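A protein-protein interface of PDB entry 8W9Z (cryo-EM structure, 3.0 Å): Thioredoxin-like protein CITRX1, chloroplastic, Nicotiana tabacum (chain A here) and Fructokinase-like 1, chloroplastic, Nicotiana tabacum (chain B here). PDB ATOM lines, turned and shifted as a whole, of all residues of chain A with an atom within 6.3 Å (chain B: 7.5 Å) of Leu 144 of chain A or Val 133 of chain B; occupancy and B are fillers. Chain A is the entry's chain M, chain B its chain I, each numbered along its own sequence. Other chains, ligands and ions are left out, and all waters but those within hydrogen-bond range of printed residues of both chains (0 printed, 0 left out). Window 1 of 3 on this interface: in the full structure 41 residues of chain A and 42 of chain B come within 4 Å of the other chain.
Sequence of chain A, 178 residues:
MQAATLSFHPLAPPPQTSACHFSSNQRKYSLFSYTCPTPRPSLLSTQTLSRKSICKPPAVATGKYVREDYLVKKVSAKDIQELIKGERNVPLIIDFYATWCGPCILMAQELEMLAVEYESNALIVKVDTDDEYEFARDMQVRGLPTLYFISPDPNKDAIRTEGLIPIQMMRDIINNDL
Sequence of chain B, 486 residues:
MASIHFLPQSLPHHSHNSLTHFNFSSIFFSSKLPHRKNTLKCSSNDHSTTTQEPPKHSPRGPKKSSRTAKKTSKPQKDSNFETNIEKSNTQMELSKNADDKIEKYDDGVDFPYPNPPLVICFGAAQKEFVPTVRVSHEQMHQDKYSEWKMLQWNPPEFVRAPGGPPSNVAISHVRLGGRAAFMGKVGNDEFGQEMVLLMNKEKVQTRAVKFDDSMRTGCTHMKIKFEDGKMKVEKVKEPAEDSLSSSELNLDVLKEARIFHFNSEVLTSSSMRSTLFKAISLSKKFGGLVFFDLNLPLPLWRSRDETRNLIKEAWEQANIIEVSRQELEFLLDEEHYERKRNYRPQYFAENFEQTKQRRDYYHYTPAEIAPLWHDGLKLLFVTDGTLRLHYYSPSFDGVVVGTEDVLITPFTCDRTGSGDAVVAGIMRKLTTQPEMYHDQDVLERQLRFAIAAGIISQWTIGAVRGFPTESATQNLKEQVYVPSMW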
ATOM      1  N   ASP A  95       0.646  11.453  22.309  1.00  0.00           N
ATOM      2  CA  ASP A  95       0.491  12.431  21.239  1.00  0.00           C
ATOM      3  C   ASP A  95       0.746  11.753  19.903  1.00  0.00           C
ATOM      4  O   ASP A  95       1.868  11.315  19.630  1.00  0.00           O
ATOM      5  CB  ASP A  95       1.449  13.611  21.433  1.00  0.00           C
ATOM      6  CG  ASP A  95       1.185  14.744  20.458  1.00  0.00           C
ATOM      7  OD1 ASP A  95       0.154  14.703  19.753  1.00  0.00           O
ATOM      8  OD2 ASP A  95       2.012  15.678  20.397  1.00  0.00           O
ATOM      9  N   PHE A  96      -0.292  11.667  19.077  1.00  0.00           N
ATOM     10  CA  PHE A  96      -0.168  11.142  17.726  1.00  0.00           C
ATOM     11  C   PHE A  96       0.245  12.260  16.780  1.00  0.00           C
ATOM     12  O   PHE A  96      -0.241  13.389  16.885  1.00  0.00           O
ATOM     13  CB  PHE A  96      -1.487  10.521  17.261  1.00  0.00           C
ATOM     14  CG  PHE A  96      -1.860   9.264  17.992  1.00  0.00           C
ATOM     15  CD1 PHE A  96      -2.495   9.321  19.221  1.00  0.00           C
ATOM     16  CD2 PHE A  96      -1.585   8.022  17.445  1.00  0.00           C
ATOM     17  CE1 PHE A  96      -2.841   8.166  19.892  1.00  0.00           C
ATOM     18  CE2 PHE A  96      -1.931   6.864  18.113  1.00  0.00           C
ATOM     19  CZ  PHE A  96      -2.558   6.936  19.338  1.00  0.00           C
ATOM     20  N   TYR A  97       1.190  11.957  15.915  1.00  0.00           N
ATOM     21  CA  TYR A  97       1.710  12.958  15.040  1.00  0.00           C
ATOM     22  C   TYR A  97       2.246  12.312  13.840  1.00  0.00           C
ATOM     23  O   TYR A  97       2.419  11.123  13.825  1.00  0.00           O
ATOM     24  CB  TYR A  97       2.856  13.656  15.730  1.00  0.00           C
ATOM     25  CG  TYR A  97       4.200  12.980  15.673  1.00  0.00           C
ATOM     26  CD1 TYR A  97       4.528  11.974  16.549  1.00  0.00           C
ATOM     27  CD2 TYR A  97       5.161  13.393  14.777  1.00  0.00           C
ATOM     28  CE1 TYR A  97       5.760  11.366  16.507  1.00  0.00           C
ATOM     29  CE2 TYR A  97       6.390  12.789  14.726  1.00  0.00           C
ATOM     30  CZ  TYR A  97       6.681  11.781  15.596  1.00  0.00           C
ATOM     31  OH  TYR A  97       7.911  11.191  15.546  1.00  0.00           O
ATOM     32  N   ALA A  98       2.466  13.076  12.802  1.00  0.00           N
ATOM     33  CA  ALA A  98       3.093  12.545  11.654  1.00  0.00           C
ATOM     34  C   ALA A  98       3.948  13.628  11.124  1.00  0.00           C
ATOM     35  O   ALA A  98       3.613  14.767  11.215  1.00  0.00           O
ATOM     36  CB  ALA A  98       2.080  12.167  10.668  1.00  0.00           C
ATOM     37  N   THR A  99       5.060  13.291  10.539  1.00  0.00           N
ATOM     38  CA  THR A  99       5.964  14.286  10.080  1.00  0.00           C
ATOM     39  C   THR A  99       5.339  15.144   9.009  1.00  0.00           C
ATOM     40  O   THR A  99       5.615  16.312   8.925  1.00  0.00           O
ATOM     41  CB  THR A  99       7.245  13.650   9.639  1.00  0.00           C
ATOM     42  OG1 THR A  99       6.967  12.704   8.610  1.00  0.00           O
ATOM     43  CG2 THR A  99       7.880  12.941  10.802  1.00  0.00           C
ATOM     44  N   TRP A 100       4.508  14.582   8.167  1.00  0.00           N
ATOM     45  CA  TRP A 100       3.839  15.345   7.136  1.00  0.00           C
ATOM     46  C   TRP A 100       2.884  16.456   7.534  1.00  0.00           C
ATOM     47  O   TRP A 100       2.799  17.424   6.820  1.00  0.00           O
ATOM     48  CB  TRP A 100       3.201  14.439   6.101  1.00  0.00           C
ATOM     49  CG  TRP A 100       2.330  13.382   6.590  1.00  0.00           C
ATOM     50  CD1 TRP A 100       2.688  12.123   6.925  1.00  0.00           C
ATOM     51  CD2 TRP A 100       0.919  13.456   6.741  1.00  0.00           C
ATOM     52  NE1 TRP A 100       1.589  11.408   7.308  1.00  0.00           N
ATOM     53  CE2 TRP A 100       0.487  12.210   7.202  1.00  0.00           C
ATOM     54  CE3 TRP A 100      -0.021  14.466   6.545  1.00  0.00           C
ATOM     55  CZ2 TRP A 100      -0.841  11.941   7.466  1.00  0.00           C
ATOM     56  CZ3 TRP A 100      -1.333  14.201   6.812  1.00  0.00           C
ATOM     57  CH2 TRP A 100      -1.735  12.951   7.265  1.00  0.00           C
ATOM     58  N   CYS A 101       2.114  16.332   8.604  1.00  0.00           N
ATOM     59  CA  CYS A 101       1.114  17.353   8.921  1.00  0.00           C
ATOM     60  C   CYS A 101       1.655  18.661   9.374  1.00  0.00           C
ATOM     61  O   CYS A 101       2.528  18.710  10.212  1.00  0.00           O
ATOM     62  CB  CYS A 101       0.160  16.896  10.003  1.00  0.00           C
ATOM     63  SG  CYS A 101       1.012  16.106  11.366  1.00  0.00           S
ATOM     64  N   CYS A 104       0.953  19.910  13.157  1.00  0.00           N
ATOM     65  CA  CYS A 104       1.769  19.239  14.122  1.00  0.00           C
ATOM     66  C   CYS A 104       2.994  19.978  14.557  1.00  0.00           C
ATOM     67  O   CYS A 104       3.404  19.837  15.687  1.00  0.00           O
ATOM     68  CB  CYS A 104       2.078  17.863  13.608  1.00  0.00           C
ATOM     69  SG  CYS A 104       0.534  17.103  13.061  1.00  0.00           S
ATOM     70  N   THR A 129       2.117   7.863  13.312  1.00  0.00           N
ATOM     71  CA  THR A 129       1.050   7.215  12.563  1.00  0.00           C
ATOM     72  C   THR A 129       1.524   6.604  11.251  1.00  0.00           C
ATOM     73  O   THR A 129       0.719   5.985  10.548  1.00  0.00           O
ATOM     74  CB  THR A 129      -0.082   8.209  12.286  1.00  0.00           C
ATOM     75  OG1 THR A 129       0.451   9.382  11.659  1.00  0.00           O
ATOM     76  CG2 THR A 129      -0.773   8.598  13.583  1.00  0.00           C
ATOM     77  N   TYR A 133       0.133   2.752  12.384  1.00  0.00           N
ATOM     78  CA  TYR A 133      -1.147   3.149  11.803  1.00  0.00           C
ATOM     79  C   TYR A 133      -2.290   2.287  12.327  1.00  0.00           C
ATOM     80  O   TYR A 133      -3.375   2.801  12.630  1.00  0.00           O
ATOM     81  CB  TYR A 133      -1.064   3.072  10.279  1.00  0.00           C
ATOM     82  CG  TYR A 133      -2.301   3.544   9.552  1.00  0.00           C
ATOM     83  CD1 TYR A 133      -2.586   4.896   9.438  1.00  0.00           C
ATOM     84  CD2 TYR A 133      -3.169   2.639   8.962  1.00  0.00           C
ATOM     85  CE1 TYR A 133      -3.711   5.333   8.768  1.00  0.00           C
ATOM     86  CE2 TYR A 133      -4.295   3.066   8.288  1.00  0.00           C
ATOM     87  CZ  TYR A 133      -4.561   4.414   8.195  1.00  0.00           C
ATOM     88  OH  TYR A 133      -5.683   4.843   7.525  1.00  0.00           O
ATOM     89  N   VAL A 141      -8.738   6.994  16.647  1.00  0.00           N
ATOM     90  CA  VAL A 141      -8.147   8.285  16.310  1.00  0.00           C
ATOM     91  C   VAL A 141      -8.636   8.693  14.926  1.00  0.00           C
ATOM     92  O   VAL A 141      -8.447   7.962  13.948  1.00  0.00           O
ATOM     93  CB  VAL A 141      -6.615   8.221  16.360  1.00  0.00           C
ATOM     94  CG1 VAL A 141      -6.014   9.546  15.953  1.00  0.00           C
ATOM     95  CG2 VAL A 141      -6.150   7.829  17.752  1.00  0.00           C
ATOM     96  N   ARG A 142      -9.268   9.863  14.839  1.00  0.00           N
ATOM     97  CA  ARG A 142      -9.801  10.370  13.580  1.00  0.00           C
ATOM     98  C   ARG A 142      -8.901  11.408  12.927  1.00  0.00           C
ATOM     99  O   ARG A 142      -8.705  11.370  11.710  1.00  0.00           O
ATOM    100  CB  ARG A 142     -11.193  10.968  13.798  1.00  0.00           C
ATOM    101  CG  ARG A 142     -12.216   9.968  14.308  1.00  0.00           C
ATOM    102  CD  ARG A 142     -13.634  10.516  14.236  1.00  0.00           C
ATOM    103  NE  ARG A 142     -13.900  11.539  15.242  1.00  0.00           N
ATOM    104  CZ  ARG A 142     -13.862  12.846  15.009  1.00  0.00           C
ATOM    105  NH1 ARG A 142     -13.566  13.299  13.799  1.00  0.00           N
ATOM    106  NH2 ARG A 142     -14.123  13.703  15.986  1.00  0.00           N
ATOM    107  N   GLY A 143      -8.311  12.325  13.656  1.00  0.00           N
ATOM    108  CA  GLY A 143      -7.534  13.367  13.009  1.00  0.00           C
ATOM    109  C   GLY A 143      -6.113  13.387  13.446  1.00  0.00           C
ATOM    110  O   GLY A 143      -5.782  12.790  14.445  1.00  0.00           O
ATOM    111  N   LEU A 144      -5.252  14.053  12.708  1.00  0.00           N
ATOM    112  CA  LEU A 144      -3.867  13.962  13.082  1.00  0.00           C
ATOM    113  C   LEU A 144      -3.403  14.550  14.373  1.00  0.00           C
ATOM    114  O   LEU A 144      -2.655  13.909  15.087  1.00  0.00           O
ATOM    115  CB  LEU A 144      -2.927  14.313  11.974  1.00  0.00           C
ATOM    116  CG  LEU A 144      -1.703  13.414  12.016  1.00  0.00           C
ATOM    117  CD1 LEU A 144      -2.052  12.033  12.538  1.00  0.00           C
ATOM    118  CD2 LEU A 144      -1.173  13.322  10.614  1.00  0.00           C
ATOM    119  N   PRO A 145      -3.835  15.760  14.717  1.00  0.00           N
ATOM    120  CA  PRO A 145      -3.341  16.176  16.039  1.00  0.00           C
ATOM    121  C   PRO A 145      -4.232  15.676  17.186  1.00  0.00           C
ATOM    122  O   PRO A 145      -5.142  16.407  17.530  1.00  0.00           O
ATOM    123  CB  PRO A 145      -3.313  17.688  15.939  1.00  0.00           C
ATOM    124  CG  PRO A 145      -3.404  17.998  14.484  1.00  0.00           C
ATOM    125  CD  PRO A 145      -4.257  16.915  13.917  1.00  0.00           C
ATOM    126  N   THR A 146      -3.991  14.501  17.771  1.00  0.00           N
ATOM    127  CA  THR A 146      -4.859  13.920  18.785  1.00  0.00           C
ATOM    128  C   THR A 146      -4.042  13.599  20.028  1.00  0.00           C
ATOM    129  O   THR A 146      -2.993  12.951  19.935  1.00  0.00           O
ATOM    130  CB  THR A 146      -5.548  12.656  18.264  1.00  0.00           C
ATOM    131  OG1 THR A 146      -6.331  12.979  17.108  1.00  0.00           O
ATOM    132  CG2 THR A 146      -6.452  12.064  19.330  1.00  0.00           C
ATOM    133  N   GLU B 128      -7.342  23.189  14.341  1.00  0.00           N
ATOM    134  CA  GLU B 128      -6.548  22.674  13.228  1.00  0.00           C
ATOM    135  C   GLU B 128      -6.714  21.162  13.211  1.00  0.00           C
ATOM    136  O   GLU B 128      -6.170  20.467  14.075  1.00  0.00           O
ATOM    137  CB  GLU B 128      -5.076  23.065  13.359  1.00  0.00           C
ATOM    138  CG  GLU B 128      -4.816  24.563  13.297  1.00  0.00           C
ATOM    139  CD  GLU B 128      -5.107  25.153  11.930  1.00  0.00           C
ATOM    140  OE1 GLU B 128      -5.082  24.400  10.933  1.00  0.00           O
ATOM    141  OE2 GLU B 128      -5.360  26.374  11.853  1.00  0.00           O
ATOM    142  N   PHE B 129      -7.462  20.656  12.235  1.00  0.00           N
ATOM    143  CA  PHE B 129      -7.847  19.252  12.204  1.00  0.00           C
ATOM    144  C   PHE B 129      -7.711  18.732  10.782  1.00  0.00           C
ATOM    145  O   PHE B 129      -8.423  19.188   9.883  1.00  0.00           O
ATOM    146  CB  PHE B 129      -9.281  19.078  12.709  1.00  0.00           C
ATOM    147  CG  PHE B 129      -9.708  17.650  12.852  1.00  0.00           C
ATOM    148  CD1 PHE B 129      -9.408  16.939  13.998  1.00  0.00           C
ATOM    149  CD2 PHE B 129     -10.424  17.023  11.847  1.00  0.00           C
ATOM    150  CE1 PHE B 129      -9.804  15.629  14.138  1.00  0.00           C
ATOM    151  CE2 PHE B 129     -10.824  15.709  11.980  1.00  0.00           C
ATOM    152  CZ  PHE B 129     -10.514  15.011  13.128  1.00  0.00           C
ATOM    153  N   VAL B 130      -6.801  17.784  10.583  1.00  0.00           N
ATOM    154  CA  VAL B 130      -6.616  17.144   9.283  1.00  0.00           C
ATOM    155  C   VAL B 130      -7.266  15.766   9.332  1.00  0.00           C
ATOM    156  O   VAL B 130      -6.693  14.831   9.910  1.00  0.00           O
ATOM    157  CB  VAL B 130      -5.129  17.048   8.913  1.00  0.00           C
ATOM    158  CG1 VAL B 130      -4.963  16.392   7.553  1.00  0.00           C
ATOM    159  CG2 VAL B 130      -4.492  18.427   8.927  1.00  0.00           C
ATOM    160  N   PRO B 131      -8.455  15.592   8.749  1.00  0.00           N
ATOM    161  CA  PRO B 131      -9.125  14.287   8.864  1.00  0.00           C
ATOM    162  C   PRO B 131      -8.481  13.200   8.025  1.00  0.00           C
ATOM    163  O   PRO B 131      -8.440  12.041   8.454  1.00  0.00           O
ATOM    164  CB  PRO B 131     -10.556  14.597   8.405  1.00  0.00           C
ATOM    165  CG  PRO B 131     -10.403  15.752   7.477  1.00  0.00           C
ATOM    166  CD  PRO B 131      -9.270  16.578   8.020  1.00  0.00           C
ATOM    167  N   THR B 132      -7.974  13.535   6.840  1.00  0.00           N
ATOM    168  CA  THR B 132      -7.379  12.543   5.947  1.00  0.00           C
ATOM    169  C   THR B 132      -5.993  12.186   6.467  1.00  0.00           C
ATOM    170  O   THR B 132      -5.034  12.939   6.288  1.00  0.00           O
ATOM    171  CB  THR B 132      -7.309  13.074   4.520  1.00  0.00           C
ATOM    172  OG1 THR B 132      -6.462  14.229   4.479  1.00  0.00           O
ATOM    173  CG2 THR B 132      -8.696  13.455   4.027  1.00  0.00           C
ATOM    174  N   VAL B 133      -5.884  11.029   7.115  1.00  0.00           N
ATOM    175  CA  VAL B 133      -4.624  10.543   7.669  1.00  0.00           C
ATOM    176  C   VAL B 133      -4.383   9.146   7.113  1.00  0.00           C
ATOM    177  O   VAL B 133      -5.124   8.209   7.435  1.00  0.00           O
ATOM    178  CB  VAL B 133      -4.629  10.523   9.202  1.00  0.00           C
ATOM    179  CG1 VAL B 133      -3.324   9.949   9.727  1.00  0.00           C
ATOM    180  CG2 VAL B 133      -4.861  11.922   9.751  1.00  0.00           C
ATOM    181  N   ARG B 134      -3.353   9.005   6.280  1.00  0.00           N
ATOM    182  CA  ARG B 134      -2.982   7.709   5.726  1.00  0.00           C
ATOM    183  C   ARG B 134      -1.507   7.428   5.988  1.00  0.00           C
ATOM    184  O   ARG B 134      -0.856   8.160   6.739  1.00  0.00           O
ATOM    185  CB  ARG B 134      -3.277   7.655   4.226  1.00  0.00           C
ATOM    186  CG  ARG B 134      -4.707   8.007   3.863  1.00  0.00           C
ATOM    187  CD  ARG B 134      -4.940   7.884   2.369  1.00  0.00           C
ATOM    188  NE  ARG B 134      -4.842   6.501   1.913  1.00  0.00           N
ATOM    189  CZ  ARG B 134      -4.988   6.118   0.650  1.00  0.00           C
ATOM    190  NH1 ARG B 134      -4.884   4.837   0.328  1.00  0.00           N
ATOM    191  NH2 ARG B 134      -5.236   7.017  -0.292  1.00  0.00           N
ATOM    192  N   VAL B 135      -0.976   6.375   5.380  1.00  0.00           N
ATOM    193  CA  VAL B 135       0.418   5.988   5.570  1.00  0.00           C
ATOM    194  C   VAL B 135       1.257   6.602   4.458  1.00  0.00           C
ATOM    195  O   VAL B 135       0.917   6.489   3.274  1.00  0.00           O
ATOM    196  CB  VAL B 135       0.565   4.459   5.592  1.00  0.00           C
ATOM    197  CG1 VAL B 135       2.002   4.070   5.900  1.00  0.00           C
ATOM    198  CG2 VAL B 135      -0.383   3.851   6.610  1.00  0.00           C
ATOM    199  N   SER B 136       2.352   7.252   4.838  1.00  0.00           N
ATOM    200  CA  SER B 136       3.275   7.867   3.896  1.00  0.00           C
ATOM    201  C   SER B 136       4.551   7.041   3.812  1.00  0.00           C
ATOM    202  O   SER B 136       5.055   6.556   4.830  1.00  0.00           O
ATOM    203  CB  SER B 136       3.608   9.303   4.308  1.00  0.00           C
ATOM    204  OG  SER B 136       4.511   9.899   3.394  1.00  0.00           O
ATOM    205  N   PHE B 158      -1.997  12.297  -1.087  1.00  0.00           N
ATOM    206  CA  PHE B 158      -3.279  12.513  -0.428  1.00  0.00           C
ATOM    207  C   PHE B 158      -3.321  13.781   0.417  1.00  0.00           C
ATOM    208  O   PHE B 158      -4.401  14.151   0.889  1.00  0.00           O
ATOM    209  CB  PHE B 158      -3.638  11.306   0.447  1.00  0.00           C
ATOM    210  CG  PHE B 158      -2.668  11.052   1.566  1.00  0.00           C
ATOM    211  CD1 PHE B 158      -1.534  10.287   1.357  1.00  0.00           C
ATOM    212  CD2 PHE B 158      -2.897  11.568   2.829  1.00  0.00           C
ATOM    213  CE1 PHE B 158      -0.645  10.050   2.385  1.00  0.00           C
ATOM    214  CE2 PHE B 158      -2.009  11.335   3.859  1.00  0.00           C
ATOM    215  CZ  PHE B 158      -0.882  10.576   3.636  1.00  0.00           C
ATOM    216  N   LEU B 296     -12.494  12.246   3.888  1.00  0.00           N
ATOM    217  CA  LEU B 296     -12.654  10.989   4.610  1.00  0.00           C
ATOM    218  C   LEU B 296     -11.729  10.926   5.820  1.00  0.00           C
ATOM    219  O   LEU B 296     -10.510  11.095   5.670  1.00  0.00           O
ATOM    220  CB  LEU B 296     -12.379   9.808   3.683  1.00  0.00           C
ATOM    221  CG  LEU B 296     -13.366   9.585   2.536  1.00  0.00           C
ATOM    222  CD1 LEU B 296     -13.006   8.331   1.759  1.00  0.00           C
ATOM    223  CD2 LEU B 296     -14.788   9.500   3.064  1.00  0.00           C
ATOM    224  N   PRO B 297     -12.255  10.690   7.023  1.00  0.00           N
ATOM    225  CA  PRO B 297     -11.389  10.579   8.206  1.00  0.00           C
ATOM    226  C   PRO B 297     -10.558   9.307   8.206  1.00  0.00           C
ATOM    227  O   PRO B 297     -10.613   8.515   7.261  1.00  0.00           O
ATOM    228  CB  PRO B 297     -12.386  10.593   9.373  1.00  0.00           C
ATOM    229  CG  PRO B 297     -13.649  11.154   8.806  1.00  0.00           C
ATOM    230  CD  PRO B 297     -13.680  10.700   7.386  1.00  0.00           C
ATOM    231  N   LEU B 298      -9.789   9.104   9.275  1.00  0.00           N
ATOM    232  CA  LEU B 298      -8.931   7.924   9.370  1.00  0.00           C
ATOM    233  C   LEU B 298      -9.708   6.611   9.344  1.00  0.00           C
ATOM    234  O   LEU B 298      -9.283   5.689   8.626  1.00  0.00           O
ATOM    235  CB  LEU B 298      -8.054   8.039  10.623  1.00  0.00           C
ATOM    236  CG  LEU B 298      -6.832   7.129  10.770  1.00  0.00           C
ATOM    237  CD1 LEU B 298      -5.780   7.811  11.626  1.00  0.00           C
ATOM    238  CD2 LEU B 298      -7.205   5.787  11.375  1.00  0.00           C
ATOM    239  N   PRO B 299     -10.814   6.438  10.081  1.00  0.00           N
ATOM    240  CA  PRO B 299     -11.517   5.145  10.032  1.00  0.00           C
ATOM    241  C   PRO B 299     -12.128   4.821   8.679  1.00  0.00           C
ATOM    242  O   PRO B 299     -12.432   3.648   8.426  1.00  0.00           O
ATOM    243  CB  PRO B 299     -12.603   5.290  11.106  1.00  0.00           C
ATOM    244  CG  PRO B 299     -12.114   6.365  12.002  1.00  0.00           C
ATOM    245  CD  PRO B 299     -11.403   7.322  11.105  1.00  0.00           C
ATOM    246  N   TRP B 301     -10.750   4.894   5.743  1.00  0.00           N
ATOM    247  CA  TRP B 301      -9.782   4.398   4.775  1.00  0.00           C
ATOM    248  C   TRP B 301      -9.465   2.919   4.962  1.00  0.00           C
ATOM    249  O   TRP B 301      -8.469   2.436   4.413  1.00  0.00           O
ATOM    250  CB  TRP B 301      -8.489   5.214   4.848  1.00  0.00           C
ATOM    251  CG  TRP B 301      -8.612   6.612   4.327  1.00  0.00           C
ATOM    252  CD1 TRP B 301      -8.774   7.748   5.060  1.00  0.00           C
ATOM    253  CD2 TRP B 301      -8.568   7.023   2.955  1.00  0.00           C
ATOM    254  NE1 TRP B 301      -8.841   8.842   4.232  1.00  0.00           N
ATOM    255  CE2 TRP B 301      -8.718   8.423   2.935  1.00  0.00           C
ATOM    256  CE3 TRP B 301      -8.422   6.343   1.743  1.00  0.00           C
ATOM    257  CZ2 TRP B 301      -8.723   9.154   1.751  1.00  0.00           C
ATOM    258  CZ3 TRP B 301      -8.427   7.072   0.571  1.00  0.00           C
ATOM    259  CH2 TRP B 301      -8.577   8.462   0.582  1.00  0.00           C
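N of Leu 144 of chain A is in hydrogen-bond range of O of Val 130 of chain B, 3.2 Å away.
The backbone carbonyl oxygen of Arg 142 of chain A sits at hydrogen-bond distance from the backbone NH of Leu 298 of chain B, 3.5 Å away.
The backbone carbonyl oxygen of Val 133 of chain B lies within hydrogen-bond range of the side-chain hydroxyl of Tyr 133 of chain A (3.4 Å).
O of Arg 142 of chain A lies close to O of Pro 131 of chain B (3.3 Å).
The backbone carbonyl oxygen (O) of Pro 131 of chain B sits at hydrogen-bond distance from the backbone NH (N) of Leu 298 of chain B, at 3.3 Å.
The indole nitrogen of Trp 301 of chain B is in hydrogen-bond range of the backbone carbonyl oxygen of Leu 296 of chain B, at 3.2 Å.
The backbone carbonyl oxygen (O) of Gly 143 of chain A sits at hydrogen-bond distance from the side-chain hydroxyl (OG1) of Thr 146 of chain A (2.7 Å).
The side-chain sulfur (SG) of Cys 104 of chain A forms a disulfide with the side-chain sulfur (SG) of Cys 101 of chain A, at 2.0 Å.
Among the printed residues, merely in contact across the chains: Val 141 of chain A with Leu 298 of chain B, Gly 143 of chain A with Phe 129 of chain B, Trp 100 of chain A with Thr 132 of chain B, Tyr 133 of chain A with Val 135 of chain B, Gly 143 of chain A with Val 130 of chain B, Arg 142 of chain A with Phe 129 of chain B, Leu 144 of chain A with Val 133 of chain B, Pro 145 of chain A with Glu 128 of chain B, Trp 100 of chain A with Phe 158 of chain B, Trp 100 of chain A with Val 133 of chain B, Trp 100 of chain A with Arg 134 of chain B, Tyr 133 of chain A with Leu 298 of chain B, Tyr 133 of chain A with Trp 301 of chain B, Tyr 133 of chain A with Arg 134 of chain B and Trp 100 of chain A with Ser 136 of chain B.
Leu 144 of chain A touches just these residues of chain B: Val 130 (3.2 Å) and Val 133 (3.7 Å).
Val 133 of chain B touches just these residues of chain A: Trp 100, Tyr 133 and Leu 144.
Printed residues of chain B within 4 Å of Arg 142 of chain A: Phe 129 (3.6 Å), Pro 131 (3.3 Å) and Leu 298 (3.5 Å).
Of the printed residues of chain A, Phe 158 of chain B touches Trp 100 (3.8 Å).
Thr 146 of chain A touches none of the printed residues of chain B.
Cys 104 of chain A touches none of the printed residues of chain B.
The nearest residue of chain A that does not touch Val 133 of chain B is Gly 143 of chain A (4.2 Å).
The nearest printed residue of chain B that does not touch Arg 142 of chain A is Pro 299 of chain B (4.2 Å).
Of the 15 printed residues of chain B, 12 touch a printed residue of chain A.
Hydrophobic or aromatic side chains of chain B within 4 Å of the printed part of chain A: Phe 129, Val 133, Val 135, Phe 158, Leu 298 and Trp 301.
Among the printed residues, no Asp or Glu carboxylate lies within 4 Å of a Lys or Arg side-chain nitrogen of the other chain.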
